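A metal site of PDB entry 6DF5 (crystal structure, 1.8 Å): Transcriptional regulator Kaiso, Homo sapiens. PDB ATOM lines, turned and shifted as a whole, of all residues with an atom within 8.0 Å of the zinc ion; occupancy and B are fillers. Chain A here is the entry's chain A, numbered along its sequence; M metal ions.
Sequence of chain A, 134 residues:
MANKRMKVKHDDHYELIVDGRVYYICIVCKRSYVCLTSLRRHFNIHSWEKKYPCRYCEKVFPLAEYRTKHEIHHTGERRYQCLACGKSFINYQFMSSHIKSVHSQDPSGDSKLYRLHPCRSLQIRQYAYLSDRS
The side-chain sulfur (SG) of Cys 85 sits close to the backbone NH (N) of Lys 87 (3.6 Å). The side-chain sulfur of Cys 82 lies close to the backbone NH of Ala 84 (3.5 Å). The backbone carbonyl oxygen (O) of Lys 87 is in hydrogen-bond range of the backbone NH (N) of Cys 82 (2.8 Å).
Within 4 Å of the zinc ion: Cys 82, Cys 85, His 98 and His 103.
The zinc ion is bound by NE2 of His 103, at 2.1 Å. SG of Cys 82 binds the zinc ion (2.1 Å). The zinc ion is bound by a ring nitrogen (NE2) of His 98, 2.1 Å away. The zinc ion is bound by SG of Cys 85 (2.3 Å).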
ATOM      1  N   GLN A  81      22.455  12.894 -18.657  1.00  0.00           N
ATOM      2  CA  GLN A  81      21.967  14.263 -18.451  1.00  0.00           C
ATOM      3  C   GLN A  81      20.445  14.329 -18.622  1.00  0.00           C
ATOM      4  O   GLN A  81      19.916  13.835 -19.609  1.00  0.00           O
ATOM      5  CB  GLN A  81      22.651  15.259 -19.404  1.00  0.00           C
ATOM      6  CG  GLN A  81      22.228  16.714 -19.119  1.00  0.00           C
ATOM      7  CD  GLN A  81      22.986  17.717 -19.959  1.00  0.00           C
ATOM      8  OE1 GLN A  81      23.486  17.370 -21.022  1.00  0.00           O
ATOM      9  NE2 GLN A  81      23.088  19.005 -19.485  1.00  0.00           N
ATOM     10  N   CYS A  82      19.788  14.878 -17.621  1.00  0.00           N
ATOM     11  CA  CYS A  82      18.357  15.201 -17.666  1.00  0.00           C
ATOM     12  C   CYS A  82      18.077  16.271 -18.713  1.00  0.00           C
ATOM     13  O   CYS A  82      18.673  17.368 -18.680  1.00  0.00           O
ATOM     14  CB  CYS A  82      17.897  15.643 -16.297  1.00  0.00           C
ATOM     15  SG  CYS A  82      16.136  16.267 -16.171  1.00  0.00           S
ATOM     16  N   LEU A  83      17.178  15.967 -19.643  1.00  0.00           N
ATOM     17  CA  LEU A  83      16.914  16.945 -20.704  1.00  0.00           C
ATOM     18  C   LEU A  83      15.918  17.998 -20.272  1.00  0.00           C
ATOM     19  O   LEU A  83      15.758  19.008 -20.953  1.00  0.00           O
ATOM     20  CB  LEU A  83      16.455  16.238 -21.975  1.00  0.00           C
ATOM     21  CG  LEU A  83      17.538  15.334 -22.571  1.00  0.00           C
ATOM     22  CD1 LEU A  83      17.077  14.676 -23.865  1.00  0.00           C
ATOM     23  CD2 LEU A  83      18.851  16.098 -22.798  1.00  0.00           C
ATOM     24  N   ALA A  84      15.254  17.788 -19.143  1.00  0.00           N
ATOM     25  CA  ALA A  84      14.265  18.741 -18.665  1.00  0.00           C
ATOM     26  C   ALA A  84      14.883  19.896 -17.862  1.00  0.00           C
ATOM     27  O   ALA A  84      14.310  20.967 -17.779  1.00  0.00           O
ATOM     28  CB  ALA A  84      13.196  18.034 -17.845  1.00  0.00           C
ATOM     29  N   CYS A  85      16.060  19.677 -17.263  1.00  0.00           N
ATOM     30  CA  CYS A  85      16.671  20.733 -16.457  1.00  0.00           C
ATOM     31  C   CYS A  85      18.194  20.829 -16.605  1.00  0.00           C
ATOM     32  O   CYS A  85      18.824  21.736 -16.054  1.00  0.00           O
ATOM     33  CB  CYS A  85      16.319  20.536 -14.985  1.00  0.00           C
ATOM     34  SG  CYS A  85      17.215  19.191 -14.176  1.00  0.00           S
ATOM     35  N   GLY A  86      18.775  19.911 -17.361  1.00  0.00           N
ATOM     36  CA  GLY A  86      20.212  19.882 -17.600  1.00  0.00           C
ATOM     37  C   GLY A  86      21.114  19.234 -16.562  1.00  0.00           C
ATOM     38  O   GLY A  86      22.318  19.072 -16.802  1.00  0.00           O
ATOM     39  N   LYS A  87      20.557  18.906 -15.392  1.00  0.00           N
ATOM     40  CA  LYS A  87      21.368  18.276 -14.349  1.00  0.00           C
ATOM     41  C   LYS A  87      21.951  16.962 -14.867  1.00  0.00           C
ATOM     42  O   LYS A  87      21.292  16.273 -15.644  1.00  0.00           O
ATOM     43  CB  LYS A  87      20.556  18.010 -13.079  1.00  0.00           C
ATOM     44  CG  LYS A  87      20.484  19.144 -12.100  1.00  0.00           C
ATOM     45  CD  LYS A  87      19.733  18.703 -10.854  1.00  0.00           C
ATOM     46  CE  LYS A  87      19.716  19.784  -9.793  1.00  0.00           C
ATOM     47  NZ  LYS A  87      21.092  20.040  -9.262  1.00  0.00           N
ATOM     48  N   SER A  88      23.172  16.645 -14.460  1.00  0.00           N
ATOM     49  CA  SER A  88      23.846  15.426 -14.927  1.00  0.00           C
ATOM     50  C   SER A  88      24.136  14.458 -13.771  1.00  0.00           C
ATOM     51  O   SER A  88      24.256  14.879 -12.613  1.00  0.00           O
ATOM     52  CB  SER A  88      25.146  15.807 -15.638  1.00  0.00           C
ATOM     53  OG  SER A  88      24.865  16.716 -16.689  1.00  0.00           O
ATOM     54  N   PHE A  89      24.276  13.174 -14.106  1.00  0.00           N
ATOM     55  CA  PHE A  89      24.320  12.112 -13.107  1.00  0.00           C
ATOM     56  C   PHE A  89      25.354  11.067 -13.524  1.00  0.00           C
ATOM     57  O   PHE A  89      25.624  10.905 -14.711  1.00  0.00           O
ATOM     58  CB  PHE A  89      22.925  11.474 -12.939  1.00  0.00           C
ATOM     59  CG  PHE A  89      21.854  12.472 -12.567  1.00  0.00           C
ATOM     60  CD1 PHE A  89      21.649  12.832 -11.245  1.00  0.00           C
ATOM     61  CD2 PHE A  89      21.117  13.117 -13.558  1.00  0.00           C
ATOM     62  CE1 PHE A  89      20.711  13.788 -10.902  1.00  0.00           C
ATOM     63  CE2 PHE A  89      20.169  14.074 -13.216  1.00  0.00           C
ATOM     64  CZ  PHE A  89      19.973  14.414 -11.892  1.00  0.00           C
ATOM     65  N   MET A  95      19.987   9.200 -12.465  1.00  0.00           N
ATOM     66  CA  MET A  95      19.228   9.887 -13.491  1.00  0.00           C
ATOM     67  C   MET A  95      17.718   9.557 -13.413  1.00  0.00           C
ATOM     68  O   MET A  95      16.864  10.449 -13.368  1.00  0.00           O
ATOM     69  CB  MET A  95      19.799   9.526 -14.877  1.00  0.00           C
ATOM     70  CG  MET A  95      19.026  10.070 -16.073  1.00  0.00           C
ATOM     71  SD  MET A  95      17.527   9.143 -16.537  1.00  0.00           S
ATOM     72  CE  MET A  95      18.202   7.543 -16.999  1.00  0.00           C
ATOM     73  N   HIS A  98      15.957  10.897 -10.347  1.00  0.00           N
ATOM     74  CA  HIS A  98      15.759  12.345 -10.462  1.00  0.00           C
ATOM     75  C   HIS A  98      14.565  12.668 -11.351  1.00  0.00           C
ATOM     76  O   HIS A  98      13.704  13.468 -10.990  1.00  0.00           O
ATOM     77  CB  HIS A  98      17.016  13.034 -11.009  1.00  0.00           C
ATOM     78  CG  HIS A  98      16.764  14.437 -11.506  1.00  0.00           C
ATOM     79  ND1 HIS A  98      16.733  15.524 -10.671  1.00  0.00           N
ATOM     80  CD2 HIS A  98      16.480  14.900 -12.744  1.00  0.00           C
ATOM     81  CE1 HIS A  98      16.450  16.612 -11.374  1.00  0.00           C
ATOM     82  NE2 HIS A  98      16.300  16.262 -12.630  1.00  0.00           N
ATOM     83  N   ILE A  99      14.480  12.024 -12.515  1.00  0.00           N
ATOM     84  CA  ILE A  99      13.424  12.345 -13.443  1.00  0.00           C
ATOM     85  C   ILE A  99      12.082  11.914 -12.879  1.00  0.00           C
ATOM     86  O   ILE A  99      11.097  12.641 -12.980  1.00  0.00           O
ATOM     87  CB  ILE A  99      13.690  11.718 -14.827  1.00  0.00           C
ATOM     88  CG1 ILE A  99      14.942  12.356 -15.433  1.00  0.00           C
ATOM     89  CG2 ILE A  99      12.545  11.946 -15.755  1.00  0.00           C
ATOM     90  CD1 ILE A  99      15.157  11.992 -16.885  1.00  0.00           C
ATOM     91  N   LYS A 100      12.043  10.739 -12.233  1.00  0.00           N
ATOM     92  CA  LYS A 100      10.827  10.259 -11.586  1.00  0.00           C
ATOM     93  C   LYS A 100      10.375  11.167 -10.435  1.00  0.00           C
ATOM     94  O   LYS A 100       9.188  11.444 -10.308  1.00  0.00           O
ATOM     95  CB  LYS A 100      11.003   8.823 -11.079  1.00  0.00           C
ATOM     96  CG  LYS A 100      10.970   7.774 -12.190  1.00  0.00           C
ATOM     97  CD  LYS A 100      11.027   6.349 -11.631  1.00  0.00           C
ATOM     98  CE  LYS A 100      10.966   5.302 -12.757  1.00  0.00           C
ATOM     99  NZ  LYS A 100      11.167   3.873 -12.276  1.00  0.00           N
ATOM    100  N   VAL A 102      11.538  14.470  -9.484  1.00  0.00           N
ATOM    101  CA  VAL A 102      11.489  15.913  -9.707  1.00  0.00           C
ATOM    102  C   VAL A 102      10.543  16.281 -10.853  1.00  0.00           C
ATOM    103  O   VAL A 102       9.825  17.292 -10.781  1.00  0.00           O
ATOM    104  CB  VAL A 102      12.899  16.466 -10.003  1.00  0.00           C
ATOM    105  CG1 VAL A 102      12.830  17.958 -10.333  1.00  0.00           C
ATOM    106  CG2 VAL A 102      13.795  16.234  -8.799  1.00  0.00           C
ATOM    107  N   HIS A 103      10.537  15.462 -11.897  1.00  0.00           N
ATOM    108  CA  HIS A 103       9.801  15.771 -13.118  1.00  0.00           C
ATOM    109  C   HIS A 103       8.537  14.903 -13.305  1.00  0.00           C
ATOM    110  O   HIS A 103       7.810  15.078 -14.267  1.00  0.00           O
ATOM    111  CB  HIS A 103      10.714  15.619 -14.326  1.00  0.00           C
ATOM    112  CG  HIS A 103      11.888  16.549 -14.308  1.00  0.00           C
ATOM    113  ND1 HIS A 103      11.734  17.919 -14.221  1.00  0.00           N
ATOM    114  CD2 HIS A 103      13.227  16.322 -14.342  1.00  0.00           C
ATOM    115  CE1 HIS A 103      12.914  18.497 -14.219  1.00  0.00           C
ATOM    116  NE2 HIS A 103      13.832  17.560 -14.303  1.00  0.00           N
ATOM    117  N   LEU A 113      13.966  11.227 -22.362  1.00  0.00           N
ATOM    118  CA  LEU A 113      14.036  12.310 -21.399  1.00  0.00           C
ATOM    119  C   LEU A 113      15.454  12.541 -20.891  1.00  0.00           C
ATOM    120  O   LEU A 113      15.678  13.358 -20.004  1.00  0.00           O
ATOM    121  CB  LEU A 113      13.132  12.009 -20.213  1.00  0.00           C
ATOM    122  CG  LEU A 113      11.657  11.736 -20.577  1.00  0.00           C
ATOM    123  CD1 LEU A 113      10.887  11.265 -19.353  1.00  0.00           C
ATOM    124  CD2 LEU A 113      11.059  12.994 -21.133  1.00  0.00           C
HETATM  125 ZN    ZN M   1      15.868  17.285 -14.398  1.00  0.00          ZN
